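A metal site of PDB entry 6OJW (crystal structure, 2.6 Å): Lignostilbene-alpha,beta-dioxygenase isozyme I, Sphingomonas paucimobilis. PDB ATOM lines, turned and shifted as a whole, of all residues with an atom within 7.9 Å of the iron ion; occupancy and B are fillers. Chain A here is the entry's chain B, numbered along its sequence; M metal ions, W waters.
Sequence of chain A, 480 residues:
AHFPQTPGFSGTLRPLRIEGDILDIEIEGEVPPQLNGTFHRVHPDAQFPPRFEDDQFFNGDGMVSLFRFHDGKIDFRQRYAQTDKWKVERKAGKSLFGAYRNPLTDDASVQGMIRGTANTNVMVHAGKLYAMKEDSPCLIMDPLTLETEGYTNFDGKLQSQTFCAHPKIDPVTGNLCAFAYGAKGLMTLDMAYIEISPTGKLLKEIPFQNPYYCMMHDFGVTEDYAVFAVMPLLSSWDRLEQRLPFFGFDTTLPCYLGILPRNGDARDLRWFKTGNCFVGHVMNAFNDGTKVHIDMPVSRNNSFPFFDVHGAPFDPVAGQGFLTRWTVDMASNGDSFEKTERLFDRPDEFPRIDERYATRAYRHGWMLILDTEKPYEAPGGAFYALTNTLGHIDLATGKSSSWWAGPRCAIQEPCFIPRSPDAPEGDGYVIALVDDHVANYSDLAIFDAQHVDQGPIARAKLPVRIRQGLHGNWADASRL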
ATOM      1  N   PHE A  58     -18.498 -28.896 -37.915  1.00  0.00           N
ATOM      2  CA  PHE A  58     -19.587 -28.057 -37.432  1.00  0.00           C
ATOM      3  C   PHE A  58     -19.953 -26.932 -38.400  1.00  0.00           C
ATOM      4  O   PHE A  58     -20.871 -26.157 -38.088  1.00  0.00           O
ATOM      5  CB  PHE A  58     -19.219 -27.454 -36.083  1.00  0.00           C
ATOM      6  CG  PHE A  58     -18.932 -28.478 -35.023  1.00  0.00           C
ATOM      7  CD1 PHE A  58     -17.636 -28.865 -34.745  1.00  0.00           C
ATOM      8  CD2 PHE A  58     -19.967 -29.060 -34.314  1.00  0.00           C
ATOM      9  CE1 PHE A  58     -17.372 -29.818 -33.769  1.00  0.00           C
ATOM     10  CE2 PHE A  58     -19.717 -30.011 -33.340  1.00  0.00           C
ATOM     11  CZ  PHE A  58     -18.419 -30.390 -33.067  1.00  0.00           C
ATOM     12  N   THR A 120     -27.354 -27.541 -35.749  1.00  0.00           N
ATOM     13  CA  THR A 120     -27.081 -28.062 -34.415  1.00  0.00           C
ATOM     14  C   THR A 120     -28.295 -28.659 -33.728  1.00  0.00           C
ATOM     15  O   THR A 120     -28.187 -29.729 -33.123  1.00  0.00           O
ATOM     16  CB  THR A 120     -26.479 -26.963 -33.528  1.00  0.00           C
ATOM     17  OG1 THR A 120     -25.326 -26.413 -34.177  1.00  0.00           O
ATOM     18  CG2 THR A 120     -26.064 -27.538 -32.177  1.00  0.00           C
ATOM     19  N   ASN A 121     -29.464 -28.019 -33.788  1.00  0.00           N
ATOM     20  CA  ASN A 121     -30.621 -28.545 -33.087  1.00  0.00           C
ATOM     21  C   ASN A 121     -31.898 -28.142 -33.793  1.00  0.00           C
ATOM     22  O   ASN A 121     -31.999 -27.077 -34.404  1.00  0.00           O
ATOM     23  CB  ASN A 121     -30.661 -28.058 -31.634  1.00  0.00           C
ATOM     24  CG  ASN A 121     -31.493 -28.962 -30.742  1.00  0.00           C
ATOM     25  OD1 ASN A 121     -32.204 -29.840 -31.220  1.00  0.00           O
ATOM     26  ND2 ASN A 121     -31.392 -28.758 -29.434  1.00  0.00           N
ATOM     27  N   GLU A 134     -25.713 -21.432 -33.129  1.00  0.00           N
ATOM     28  CA  GLU A 134     -25.310 -20.435 -32.130  1.00  0.00           C
ATOM     29  C   GLU A 134     -25.128 -19.043 -32.728  1.00  0.00           C
ATOM     30  O   GLU A 134     -25.538 -18.043 -32.121  1.00  0.00           O
ATOM     31  CB  GLU A 134     -24.002 -20.857 -31.461  1.00  0.00           C
ATOM     32  CG  GLU A 134     -24.161 -21.838 -30.346  1.00  0.00           C
ATOM     33  CD  GLU A 134     -22.890 -22.590 -30.113  1.00  0.00           C
ATOM     34  OE1 GLU A 134     -21.812 -21.966 -30.141  1.00  0.00           O
ATOM     35  OE2 GLU A 134     -22.972 -23.809 -29.918  1.00  0.00           O
ATOM     36  N   ALA A 165     -28.707 -22.906 -29.423  1.00  0.00           N
ATOM     37  CA  ALA A 165     -29.216 -24.147 -29.980  1.00  0.00           C
ATOM     38  C   ALA A 165     -29.563 -25.170 -28.896  1.00  0.00           C
ATOM     39  O   ALA A 165     -29.757 -26.354 -29.215  1.00  0.00           O
ATOM     40  CB  ALA A 165     -28.215 -24.749 -30.960  1.00  0.00           C
ATOM     41  N   HIS A 166     -29.645 -24.753 -27.636  1.00  0.00           N
ATOM     42  CA  HIS A 166     -29.894 -25.657 -26.525  1.00  0.00           C
ATOM     43  C   HIS A 166     -30.936 -25.065 -25.574  1.00  0.00           C
ATOM     44  O   HIS A 166     -30.683 -24.908 -24.382  1.00  0.00           O
ATOM     45  CB  HIS A 166     -28.596 -25.965 -25.780  1.00  0.00           C
ATOM     46  CG  HIS A 166     -27.789 -27.044 -26.420  1.00  0.00           C
ATOM     47  ND1 HIS A 166     -28.228 -28.352 -26.452  1.00  0.00           N
ATOM     48  CD2 HIS A 166     -26.602 -27.026 -27.068  1.00  0.00           C
ATOM     49  CE1 HIS A 166     -27.330 -29.093 -27.085  1.00  0.00           C
ATOM     50  NE2 HIS A 166     -26.340 -28.319 -27.465  1.00  0.00           N
ATOM     51  N   HIS A 217     -22.118 -22.704 -25.374  1.00  0.00           N
ATOM     52  CA  HIS A 217     -22.883 -23.655 -26.179  1.00  0.00           C
ATOM     53  C   HIS A 217     -24.182 -24.057 -25.483  1.00  0.00           C
ATOM     54  O   HIS A 217     -25.256 -24.010 -26.094  1.00  0.00           O
ATOM     55  CB  HIS A 217     -22.033 -24.895 -26.462  1.00  0.00           C
ATOM     56  CG  HIS A 217     -22.715 -25.921 -27.316  1.00  0.00           C
ATOM     57  ND1 HIS A 217     -23.185 -25.642 -28.581  1.00  0.00           N
ATOM     58  CD2 HIS A 217     -23.012 -27.221 -27.092  1.00  0.00           C
ATOM     59  CE1 HIS A 217     -23.737 -26.723 -29.094  1.00  0.00           C
ATOM     60  NE2 HIS A 217     -23.643 -27.697 -28.221  1.00  0.00           N
ATOM     61  N   ASP A 218     -24.098 -24.438 -24.216  1.00  0.00           N
ATOM     62  CA  ASP A 218     -25.248 -24.953 -23.497  1.00  0.00           C
ATOM     63  C   ASP A 218     -25.388 -24.198 -22.185  1.00  0.00           C
ATOM     64  O   ASP A 218     -24.469 -23.509 -21.726  1.00  0.00           O
ATOM     65  CB  ASP A 218     -25.110 -26.459 -23.227  1.00  0.00           C
ATOM     66  CG  ASP A 218     -26.450 -27.149 -23.012  1.00  0.00           C
ATOM     67  OD1 ASP A 218     -27.472 -26.453 -22.813  1.00  0.00           O
ATOM     68  OD2 ASP A 218     -26.462 -28.393 -23.053  1.00  0.00           O
ATOM     69  N   GLY A 280     -19.183 -29.681 -20.975  1.00  0.00           N
ATOM     70  CA  GLY A 280     -19.953 -30.206 -22.077  1.00  0.00           C
ATOM     71  C   GLY A 280     -21.438 -29.962 -21.950  1.00  0.00           C
ATOM     72  O   GLY A 280     -21.871 -28.994 -21.306  1.00  0.00           O
ATOM     73  N   HIS A 281     -22.240 -30.837 -22.561  1.00  0.00           N
ATOM     74  CA  HIS A 281     -23.671 -30.630 -22.621  1.00  0.00           C
ATOM     75  C   HIS A 281     -24.320 -30.787 -21.244  1.00  0.00           C
ATOM     76  O   HIS A 281     -23.851 -31.550 -20.396  1.00  0.00           O
ATOM     77  CB  HIS A 281     -24.297 -31.621 -23.607  1.00  0.00           C
ATOM     78  CG  HIS A 281     -24.013 -31.283 -25.044  1.00  0.00           C
ATOM     79  ND1 HIS A 281     -23.086 -31.962 -25.795  1.00  0.00           N
ATOM     80  CD2 HIS A 281     -24.527 -30.322 -25.848  1.00  0.00           C
ATOM     81  CE1 HIS A 281     -23.043 -31.441 -27.014  1.00  0.00           C
ATOM     82  NE2 HIS A 281     -23.904 -30.447 -27.070  1.00  0.00           N
ATOM     83  N   VAL A 282     -25.410 -30.066 -21.048  1.00  0.00           N
ATOM     84  CA  VAL A 282     -26.121 -30.068 -19.770  1.00  0.00           C
ATOM     85  C   VAL A 282     -27.180 -31.170 -19.794  1.00  0.00           C
ATOM     86  O   VAL A 282     -28.102 -31.136 -20.614  1.00  0.00           O
ATOM     87  CB  VAL A 282     -26.766 -28.696 -19.500  1.00  0.00           C
ATOM     88  CG1 VAL A 282     -27.598 -28.741 -18.214  1.00  0.00           C
ATOM     89  CG2 VAL A 282     -25.702 -27.621 -19.423  1.00  0.00           C
ATOM     90  N   PHE A 304     -15.486 -32.293 -27.455  1.00  0.00           N
ATOM     91  CA  PHE A 304     -16.565 -32.247 -28.433  1.00  0.00           C
ATOM     92  C   PHE A 304     -16.286 -33.078 -29.670  1.00  0.00           C
ATOM     93  O   PHE A 304     -17.200 -33.691 -30.215  1.00  0.00           O
ATOM     94  CB  PHE A 304     -16.842 -30.788 -28.855  1.00  0.00           C
ATOM     95  CG  PHE A 304     -17.856 -30.065 -27.991  1.00  0.00           C
ATOM     96  CD1 PHE A 304     -18.370 -30.626 -26.832  1.00  0.00           C
ATOM     97  CD2 PHE A 304     -18.292 -28.796 -28.361  1.00  0.00           C
ATOM     98  CE1 PHE A 304     -19.293 -29.952 -26.069  1.00  0.00           C
ATOM     99  CE2 PHE A 304     -19.214 -28.122 -27.597  1.00  0.00           C
ATOM    100  CZ  PHE A 304     -19.714 -28.692 -26.448  1.00  0.00           C
ATOM    101  N   GLU A 349     -21.149 -38.420 -23.032  1.00  0.00           N
ATOM    102  CA  GLU A 349     -21.608 -37.134 -23.549  1.00  0.00           C
ATOM    103  C   GLU A 349     -23.039 -37.304 -24.046  1.00  0.00           C
ATOM    104  O   GLU A 349     -23.660 -38.350 -23.852  1.00  0.00           O
ATOM    105  CB  GLU A 349     -20.671 -36.630 -24.645  1.00  0.00           C
ATOM    106  CG  GLU A 349     -19.982 -35.313 -24.302  1.00  0.00           C
ATOM    107  CD  GLU A 349     -20.943 -34.148 -24.186  1.00  0.00           C
ATOM    108  OE1 GLU A 349     -22.094 -34.253 -24.682  1.00  0.00           O
ATOM    109  OE2 GLU A 349     -20.555 -33.111 -23.607  1.00  0.00           O
ATOM    110  N   PHE A 350     -23.555 -36.262 -24.692  1.00  0.00           N
ATOM    111  CA  PHE A 350     -24.926 -36.245 -25.201  1.00  0.00           C
ATOM    112  C   PHE A 350     -25.921 -36.752 -24.165  1.00  0.00           C
ATOM    113  O   PHE A 350     -26.627 -37.766 -24.406  1.00  0.00           O
ATOM    114  CB  PHE A 350     -25.016 -37.035 -26.489  1.00  0.00           C
ATOM    115  CG  PHE A 350     -24.337 -36.358 -27.643  1.00  0.00           C
ATOM    116  CD1 PHE A 350     -24.988 -35.376 -28.365  1.00  0.00           C
ATOM    117  CD2 PHE A 350     -23.030 -36.669 -27.962  1.00  0.00           C
ATOM    118  CE1 PHE A 350     -24.355 -34.730 -29.415  1.00  0.00           C
ATOM    119  CE2 PHE A 350     -22.392 -36.037 -29.011  1.00  0.00           C
ATOM    120  CZ  PHE A 350     -23.058 -35.061 -29.729  1.00  0.00           C
ATOM    121  N   GLU A 413     -27.179 -39.285 -30.834  1.00  0.00           N
ATOM    122  CA  GLU A 413     -27.782 -38.813 -29.598  1.00  0.00           C
ATOM    123  C   GLU A 413     -29.119 -39.516 -29.365  1.00  0.00           C
ATOM    124  O   GLU A 413     -29.960 -39.550 -30.263  1.00  0.00           O
ATOM    125  CB  GLU A 413     -28.007 -37.304 -29.634  1.00  0.00           C
ATOM    126  CG  GLU A 413     -28.567 -36.757 -28.327  1.00  0.00           C
ATOM    127  CD  GLU A 413     -29.145 -35.371 -28.473  1.00  0.00           C
ATOM    128  OE1 GLU A 413     -30.053 -35.193 -29.312  1.00  0.00           O
ATOM    129  OE2 GLU A 413     -28.691 -34.470 -27.749  1.00  0.00           O
ATOM    130  N   LEU A 470     -26.202 -34.169 -34.711  1.00  0.00           N
ATOM    131  CA  LEU A 470     -26.050 -33.476 -33.440  1.00  0.00           C
ATOM    132  C   LEU A 470     -27.267 -33.777 -32.603  1.00  0.00           C
ATOM    133  O   LEU A 470     -27.394 -34.887 -32.057  1.00  0.00           O
ATOM    134  CB  LEU A 470     -25.783 -31.982 -33.694  1.00  0.00           C
ATOM    135  CG  LEU A 470     -24.381 -31.724 -34.264  1.00  0.00           C
ATOM    136  CD1 LEU A 470     -24.221 -30.307 -34.777  1.00  0.00           C
ATOM    137  CD2 LEU A 470     -23.321 -32.022 -33.211  1.00  0.00           C
ATOM    138  N   HIS A 471     -28.216 -32.853 -32.479  1.00  0.00           N
ATOM    139  CA  HIS A 471     -29.298 -32.977 -31.517  1.00  0.00           C
ATOM    140  C   HIS A 471     -30.635 -33.160 -32.206  1.00  0.00           C
ATOM    141  O   HIS A 471     -30.888 -32.637 -33.293  1.00  0.00           O
ATOM    142  CB  HIS A 471     -29.337 -31.748 -30.598  1.00  0.00           C
ATOM    143  CG  HIS A 471     -28.033 -31.487 -29.911  1.00  0.00           C
ATOM    144  ND1 HIS A 471     -27.554 -32.286 -28.893  1.00  0.00           N
ATOM    145  CD2 HIS A 471     -27.106 -30.518 -30.109  1.00  0.00           C
ATOM    146  CE1 HIS A 471     -26.383 -31.822 -28.494  1.00  0.00           C
ATOM    147  NE2 HIS A 471     -26.084 -30.761 -29.205  1.00  0.00           N
HETATM  148 FE    FE M   1     -24.711 -29.256 -28.698  1.00  0.00          FE
HETATM  149  O   HOH W   1     -22.951 -29.807 -30.372  1.00  0.00           O
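N of His 471 is in hydrogen-bond range of O of Thr 120.
ND1 of His 471 is in hydrogen-bond range of OE2 of Glu 413.
The side-chain carboxylate (OE1) of Glu 349 sits at hydrogen-bond distance from a ring nitrogen (ND1) of His 281 (2.7 Å).
Four residues have an atom within 4 Å of the iron ion: His 166, His 217, His 281 and His 471.
The iron ion is bound by a ring nitrogen (NE2) of His 217 (1.9 Å), a ring nitrogen (NE2) of His 471 (2.1 Å), a ring nitrogen (NE2) of His 281 (2.2 Å), a ring nitrogen (NE2) of His 166 (2.2 Å) and water W1 (2.5 Å).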
